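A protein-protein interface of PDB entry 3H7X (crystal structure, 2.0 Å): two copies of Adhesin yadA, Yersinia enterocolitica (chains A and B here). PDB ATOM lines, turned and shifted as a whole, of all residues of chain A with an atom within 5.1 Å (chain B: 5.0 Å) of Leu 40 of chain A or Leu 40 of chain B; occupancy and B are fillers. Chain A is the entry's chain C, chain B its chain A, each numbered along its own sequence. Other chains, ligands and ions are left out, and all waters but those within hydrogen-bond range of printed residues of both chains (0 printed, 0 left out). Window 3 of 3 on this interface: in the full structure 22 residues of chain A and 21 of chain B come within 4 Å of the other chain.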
ATOM      1  N   LYS A  36      15.574 -26.586 -27.267  1.00  0.00           N
ATOM      2  CA  LYS A  36      16.340 -26.018 -26.151  1.00  0.00           C
ATOM      3  C   LYS A  36      16.156 -24.499 -26.124  1.00  0.00           C
ATOM      4  O   LYS A  36      15.949 -23.873 -25.060  1.00  0.00           O
ATOM      5  CB  LYS A  36      17.858 -26.275 -26.193  1.00  0.00           C
ATOM      6  CG  LYS A  36      18.622 -27.675 -25.793  1.00  0.00           C
ATOM      7  CD  LYS A  36      18.009 -28.581 -24.789  1.00  0.00           C
ATOM      8  CE  LYS A  36      17.990 -27.878 -23.402  1.00  0.00           C
ATOM      9  NZ  LYS A  36      17.991 -28.958 -22.345  1.00  0.00           N
ATOM     10  N   PHE A  37      16.262 -23.886 -27.325  1.00  0.00           N
ATOM     11  CA  PHE A  37      16.191 -22.416 -27.529  1.00  0.00           C
ATOM     12  C   PHE A  37      14.937 -21.944 -26.780  1.00  0.00           C
ATOM     13  O   PHE A  37      14.899 -20.950 -26.016  1.00  0.00           O
ATOM     14  CB  PHE A  37      16.028 -22.117 -29.051  1.00  0.00           C
ATOM     15  CG  PHE A  37      16.018 -20.645 -29.430  1.00  0.00           C
ATOM     16  CD1 PHE A  37      17.203 -19.912 -29.473  1.00  0.00           C
ATOM     17  CD2 PHE A  37      14.830 -20.037 -29.901  1.00  0.00           C
ATOM     18  CE1 PHE A  37      17.174 -18.505 -29.874  1.00  0.00           C
ATOM     19  CE2 PHE A  37      14.814 -18.640 -30.287  1.00  0.00           C
ATOM     20  CZ  PHE A  37      15.984 -17.904 -30.282  1.00  0.00           C
ATOM     21  N   HIS A  38      13.886 -22.674 -27.066  1.00  0.00           N
ATOM     22  CA  HIS A  38      12.583 -22.367 -26.677  1.00  0.00           C
ATOM     23  C   HIS A  38      12.310 -22.375 -25.206  1.00  0.00           C
ATOM     24  O   HIS A  38      11.562 -21.516 -24.703  1.00  0.00           O
ATOM     25  CB  HIS A  38      11.825 -23.500 -27.128  1.00  0.00           C
ATOM     26  CG  HIS A  38      10.807 -23.165 -28.096  1.00  0.00           C
ATOM     27  ND1 HIS A  38       9.513 -22.944 -27.706  1.00  0.00           N
ATOM     28  CD2 HIS A  38      10.870 -22.991 -29.442  1.00  0.00           C
ATOM     29  CE1 HIS A  38       8.800 -22.670 -28.796  1.00  0.00           C
ATOM     30  NE2 HIS A  38       9.608 -22.694 -29.861  1.00  0.00           N
ATOM     31  N   GLN A  39      12.842 -23.420 -24.577  1.00  0.00           N
ATOM     32  CA  GLN A  39      12.906 -23.531 -23.140  1.00  0.00           C
ATOM     33  C   GLN A  39      13.519 -22.275 -22.584  1.00  0.00           C
ATOM     34  O   GLN A  39      12.939 -21.646 -21.709  1.00  0.00           O
ATOM     35  CB  GLN A  39      13.747 -24.742 -22.728  1.00  0.00           C
ATOM     36  CG  GLN A  39      13.386 -26.096 -23.328  1.00  0.00           C
ATOM     37  CD  GLN A  39      14.059 -27.197 -22.465  1.00  0.00           C
ATOM     38  OE1 GLN A  39      13.432 -27.760 -21.595  1.00  0.00           O
ATOM     39  NE2 GLN A  39      15.347 -27.371 -22.618  1.00  0.00           N
ATOM     40  N   LEU A  40      14.687 -21.915 -23.109  1.00  0.00           N
ATOM     41  CA  LEU A  40      15.391 -20.746 -22.682  1.00  0.00           C
ATOM     42  C   LEU A  40      14.708 -19.404 -22.938  1.00  0.00           C
ATOM     43  O   LEU A  40      14.731 -18.498 -22.097  1.00  0.00           O
ATOM     44  CB  LEU A  40      16.853 -20.706 -23.171  1.00  0.00           C
ATOM     45  CG  LEU A  40      17.780 -21.698 -22.464  1.00  0.00           C
ATOM     46  CD1 LEU A  40      19.028 -21.862 -23.345  1.00  0.00           C
ATOM     47  CD2 LEU A  40      18.144 -21.286 -21.016  1.00  0.00           C
ATOM     48  N   ASP A  41      14.119 -19.267 -24.095  1.00  0.00           N
ATOM     49  CA  ASP A  41      13.253 -18.134 -24.411  1.00  0.00           C
ATOM     50  C   ASP A  41      12.071 -17.940 -23.452  1.00  0.00           C
ATOM     51  O   ASP A  41      11.745 -16.825 -23.117  1.00  0.00           O
ATOM     52  CB  ASP A  41      12.611 -18.377 -25.764  1.00  0.00           C
ATOM     53  CG  ASP A  41      12.839 -17.280 -26.715  1.00  0.00           C
ATOM     54  OD1 ASP A  41      13.873 -16.540 -26.662  1.00  0.00           O
ATOM     55  OD2 ASP A  41      11.967 -17.217 -27.609  1.00  0.00           O
ATOM     56  N   ASN A  42      11.347 -19.003 -23.150  1.00  0.00           N
ATOM     57  CA  ASN A  42      10.248 -18.961 -22.223  1.00  0.00           C
ATOM     58  C   ASN A  42      10.733 -18.570 -20.825  1.00  0.00           C
ATOM     59  O   ASN A  42      10.022 -17.848 -20.156  1.00  0.00           O
ATOM     60  CB  ASN A  42       9.502 -20.271 -22.175  1.00  0.00           C
ATOM     61  CG  ASN A  42       8.274 -20.326 -23.137  1.00  0.00           C
ATOM     62  OD1 ASN A  42       8.144 -19.528 -24.098  1.00  0.00           O
ATOM     63  ND2 ASN A  42       7.369 -21.282 -22.891  1.00  0.00           N
ATOM     64  N   ARG A  43      11.911 -19.040 -20.383  1.00  0.00           N
ATOM     65  CA  ARG A  43      12.559 -18.476 -19.125  1.00  0.00           C
ATOM     66  C   ARG A  43      12.956 -16.951 -19.145  1.00  0.00           C
ATOM     67  O   ARG A  43      12.691 -16.164 -18.221  1.00  0.00           O
ATOM     68  CB  ARG A  43      13.669 -19.401 -18.623  1.00  0.00           C
ATOM     69  CG  ARG A  43      13.077 -20.434 -17.618  1.00  0.00           C
ATOM     70  CD  ARG A  43      13.969 -21.102 -16.535  1.00  0.00           C
ATOM     71  NE  ARG A  43      15.017 -20.309 -15.907  1.00  0.00           N
ATOM     72  CZ  ARG A  43      16.324 -20.484 -16.074  1.00  0.00           C
ATOM     73  NH1 ARG A  43      16.822 -21.334 -16.943  1.00  0.00           N
ATOM     74  NH2 ARG A  43      17.158 -19.795 -15.383  1.00  0.00           N
ATOM     75  N   LEU A  44      13.534 -16.519 -20.252  1.00  0.00           N
ATOM     76  CA  LEU A  44      13.817 -15.138 -20.450  1.00  0.00           C
ATOM     77  C   LEU A  44      12.598 -14.218 -20.404  1.00  0.00           C
ATOM     78  O   LEU A  44      12.693 -13.176 -19.750  1.00  0.00           O
ATOM     79  CB  LEU A  44      14.609 -14.923 -21.734  1.00  0.00           C
ATOM     80  CG  LEU A  44      16.096 -14.927 -21.646  1.00  0.00           C
ATOM     81  CD1 LEU A  44      16.584 -14.614 -23.032  1.00  0.00           C
ATOM     82  CD2 LEU A  44      16.519 -13.820 -20.649  1.00  0.00           C
ATOM     83  N   LYS B  36      21.894 -19.675 -32.481  1.00  0.00           N
ATOM     84  CA  LYS B  36      20.796 -19.492 -31.517  1.00  0.00           C
ATOM     85  C   LYS B  36      21.209 -19.126 -30.055  1.00  0.00           C
ATOM     86  O   LYS B  36      20.534 -18.358 -29.412  1.00  0.00           O
ATOM     87  CB  LYS B  36      19.904 -20.754 -31.502  1.00  0.00           C
ATOM     88  CG  LYS B  36      19.034 -20.985 -32.755  1.00  0.00           C
ATOM     89  CD  LYS B  36      17.994 -19.967 -32.940  1.00  0.00           C
ATOM     90  CE  LYS B  36      16.678 -20.520 -32.534  1.00  0.00           C
ATOM     91  NZ  LYS B  36      15.559 -20.017 -33.361  1.00  0.00           N
ATOM     92  N   PHE B  37      22.279 -19.677 -29.535  1.00  0.00           N
ATOM     93  CA  PHE B  37      22.877 -19.371 -28.255  1.00  0.00           C
ATOM     94  C   PHE B  37      23.146 -17.847 -28.162  1.00  0.00           C
ATOM     95  O   PHE B  37      22.981 -17.209 -27.101  1.00  0.00           O
ATOM     96  CB  PHE B  37      24.246 -20.081 -28.307  1.00  0.00           C
ATOM     97  CG  PHE B  37      25.217 -19.814 -27.108  1.00  0.00           C
ATOM     98  CD1 PHE B  37      25.332 -20.773 -26.084  1.00  0.00           C
ATOM     99  CD2 PHE B  37      26.103 -18.721 -27.087  1.00  0.00           C
ATOM    100  CE1 PHE B  37      26.275 -20.610 -25.038  1.00  0.00           C
ATOM    101  CE2 PHE B  37      27.006 -18.550 -26.053  1.00  0.00           C
ATOM    102  CZ  PHE B  37      27.089 -19.514 -25.020  1.00  0.00           C
ATOM    103  N   HIS B  38      23.661 -17.307 -29.288  1.00  0.00           N
ATOM    104  CA  HIS B  38      24.116 -15.954 -29.414  1.00  0.00           C
ATOM    105  C   HIS B  38      22.967 -14.988 -29.260  1.00  0.00           C
ATOM    106  O   HIS B  38      23.099 -13.944 -28.595  1.00  0.00           O
ATOM    107  CB  HIS B  38      24.527 -15.814 -30.845  1.00  0.00           C
ATOM    108  CG  HIS B  38      25.830 -15.190 -31.015  1.00  0.00           C
ATOM    109  ND1 HIS B  38      25.986 -13.822 -31.088  1.00  0.00           N
ATOM    110  CD2 HIS B  38      27.070 -15.726 -31.127  1.00  0.00           C
ATOM    111  CE1 HIS B  38      27.264 -13.546 -31.277  1.00  0.00           C
ATOM    112  NE2 HIS B  38      27.943 -14.677 -31.293  1.00  0.00           N
ATOM    113  N   GLN B  39      21.837 -15.277 -29.938  1.00  0.00           N
ATOM    114  CA  GLN B  39      20.658 -14.465 -29.753  1.00  0.00           C
ATOM    115  C   GLN B  39      20.239 -14.458 -28.261  1.00  0.00           C
ATOM    116  O   GLN B  39      19.899 -13.369 -27.710  1.00  0.00           O
ATOM    117  CB  GLN B  39      19.503 -14.820 -30.662  1.00  0.00           C
ATOM    118  CG  GLN B  39      19.712 -14.584 -32.195  1.00  0.00           C
ATOM    119  CD  GLN B  39      18.634 -15.322 -32.999  1.00  0.00           C
ATOM    120  OE1 GLN B  39      17.962 -14.752 -33.884  1.00  0.00           O
ATOM    121  NE2 GLN B  39      18.467 -16.592 -32.706  1.00  0.00           N
ATOM    122  N   LEU B  40      20.220 -15.635 -27.623  1.00  0.00           N
ATOM    123  CA  LEU B  40      20.031 -15.720 -26.155  1.00  0.00           C
ATOM    124  C   LEU B  40      21.049 -15.010 -25.287  1.00  0.00           C
ATOM    125  O   LEU B  40      20.644 -14.469 -24.275  1.00  0.00           O
ATOM    126  CB  LEU B  40      19.925 -17.171 -25.695  1.00  0.00           C
ATOM    127  CG  LEU B  40      18.655 -17.884 -26.152  1.00  0.00           C
ATOM    128  CD1 LEU B  40      18.767 -19.391 -26.009  1.00  0.00           C
ATOM    129  CD2 LEU B  40      17.401 -17.292 -25.452  1.00  0.00           C
ATOM    130  N   ASP B  41      22.334 -15.026 -25.664  1.00  0.00           N
ATOM    131  CA  ASP B  41      23.371 -14.329 -24.966  1.00  0.00           C
ATOM    132  C   ASP B  41      23.095 -12.863 -24.989  1.00  0.00           C
ATOM    133  O   ASP B  41      23.274 -12.194 -23.957  1.00  0.00           O
ATOM    134  CB  ASP B  41      24.752 -14.525 -25.635  1.00  0.00           C
ATOM    135  CG  ASP B  41      25.779 -14.886 -24.681  1.00  0.00           C
ATOM    136  OD1 ASP B  41      25.389 -15.400 -23.587  1.00  0.00           O
ATOM    137  OD2 ASP B  41      27.004 -14.692 -24.983  1.00  0.00           O
ATOM    138  N   ASN B  42      22.758 -12.367 -26.196  1.00  0.00           N
ATOM    139  CA  ASN B  42      22.522 -10.932 -26.393  1.00  0.00           C
ATOM    140  C   ASN B  42      21.377 -10.543 -25.517  1.00  0.00           C
ATOM    141  O   ASN B  42      21.485  -9.539 -24.861  1.00  0.00           O
ATOM    142  CB  ASN B  42      22.281 -10.514 -27.858  1.00  0.00           C
ATOM    143  CG  ASN B  42      23.542 -10.318 -28.689  1.00  0.00           C
ATOM    144  OD1 ASN B  42      24.692 -10.384 -28.250  1.00  0.00           O
ATOM    145  ND2 ASN B  42      23.302 -10.035 -29.955  1.00  0.00           N
ATOM    146  N   ARG B  43      20.278 -11.284 -25.501  1.00  0.00           N
ATOM    147  CA  ARG B  43      19.142 -10.930 -24.639  1.00  0.00           C
ATOM    148  C   ARG B  43      19.492 -10.928 -23.134  1.00  0.00           C
ATOM    149  O   ARG B  43      19.071 -10.014 -22.408  1.00  0.00           O
ATOM    150  CB  ARG B  43      17.923 -11.831 -24.942  1.00  0.00           C
ATOM    151  CG  ARG B  43      16.586 -11.135 -25.093  1.00  0.00           C
ATOM    152  CD  ARG B  43      15.526 -12.195 -25.248  1.00  0.00           C
ATOM    153  NE  ARG B  43      14.228 -11.811 -24.785  1.00  0.00           N
ATOM    154  CZ  ARG B  43      13.256 -12.640 -24.552  1.00  0.00           C
ATOM    155  NH1 ARG B  43      13.472 -13.969 -24.684  1.00  0.00           N
ATOM    156  NH2 ARG B  43      12.090 -12.175 -24.174  1.00  0.00           N
ATOM    157  N   LEU B  44      20.249 -11.923 -22.668  1.00  0.00           N
ATOM    158  CA  LEU B  44      20.751 -11.923 -21.276  1.00  0.00           C
ATOM    159  C   LEU B  44      21.673 -10.766 -20.934  1.00  0.00           C
ATOM    160  O   LEU B  44      21.593 -10.172 -19.825  1.00  0.00           O
ATOM    161  CB  LEU B  44      21.510 -13.166 -21.010  1.00  0.00           C
ATOM    162  CG  LEU B  44      20.889 -14.393 -20.350  1.00  0.00           C
ATOM    163  CD1 LEU B  44      22.068 -15.177 -20.084  1.00  0.00           C
ATOM    164  CD2 LEU B  44      20.164 -14.099 -19.053  1.00  0.00           C
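The side-chain carboxylate (OD1) of Asp 41 of chain A lies within salt-bridge range of the guanidinium group (NH1) of Arg 43 of chain B.
Phe 37 of chain A touches Lys 36 of chain B (CD1 to CE, 3.2 Å). NE2 of Gln 39 of chain B touches CE1 of Phe 37 of chain A, 3.7 Å away. Leu 40 of chain B touches Phe 37 of chain A (CD1 to CD1, 3.8 Å). Leu 40 of chain B touches Leu 40 of chain A (CD1 to CD1, 3.6 Å). Asp 41 of chain A touches Leu 40 of chain B (OD1 to CD2, 3.8 Å). Leu 44 of chain A touches Leu 40 of chain B. Arg 43 of chain B touches Leu 44 of chain A (NH1 to CB, 3.3 Å). Leu 44 of chain B touches Leu 44 of chain A (CD2 to CD2, 3.99 Å).
Printed residues of chain B within 4 Å of Leu 40 of chain A: Leu 40. Leu 40 of chain B touches four residues of chain A. Of the printed residues of chain A, Lys 36 of chain B touches Phe 37 (3.2 Å). Of the printed residues of chain A, Arg 43 of chain B touches Asp 41 (3.3 Å) and Leu 44 (3.3 Å). Of the printed residues of chain A, Leu 44 of chain B touches Leu 44 (3.99 Å). Of the printed residues of chain B, Phe 37 of chain A touches Lys 36 (3.2 Å), Gln 39 (3.7 Å) and Leu 40 (3.8 Å). Arg 43 of chain A touches none of the printed residues of chain B. The nearest printed residue of chain A that does not touch Leu 40 of chain B is Lys 36 of chain A (5.4 Å).
Of the 9 printed residues of chain A, 4 touch a printed residue of chain B. Hydrophobic or aromatic side chains of chain A within 4 Å of the printed part of chain B: Phe 37, Leu 40 and Leu 44. Hydrophobic or aromatic side chains of chain B that line the printed part of chain A: Leu 40 and Leu 44. Along chain B the printed residues that touch a printed residue of chain A span positions 36 to 44.
Phe 37 of chain A touches Lys 36 of chain B, but with the chains exchanged Lys 36 of chain A does not touch Phe 37 of chain B (8.5 Å). Asp 41 of chain A touches Leu 40 of chain B, but with the chains exchanged Leu 40 of chain A does not touch Asp 41 of chain B (7.9 Å). Leu 44 of chain A touches Leu 40 of chain B, but with the chains exchanged Leu 40 of chain A does not touch Leu 44 of chain B (7.3 Å). Leu 44 of chain A touches its own counterpart, Leu 44 of chain B. Of the 9 pairs that touch across the chains among the printed residues, 2 have their exchanged pair printed and touching as well.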
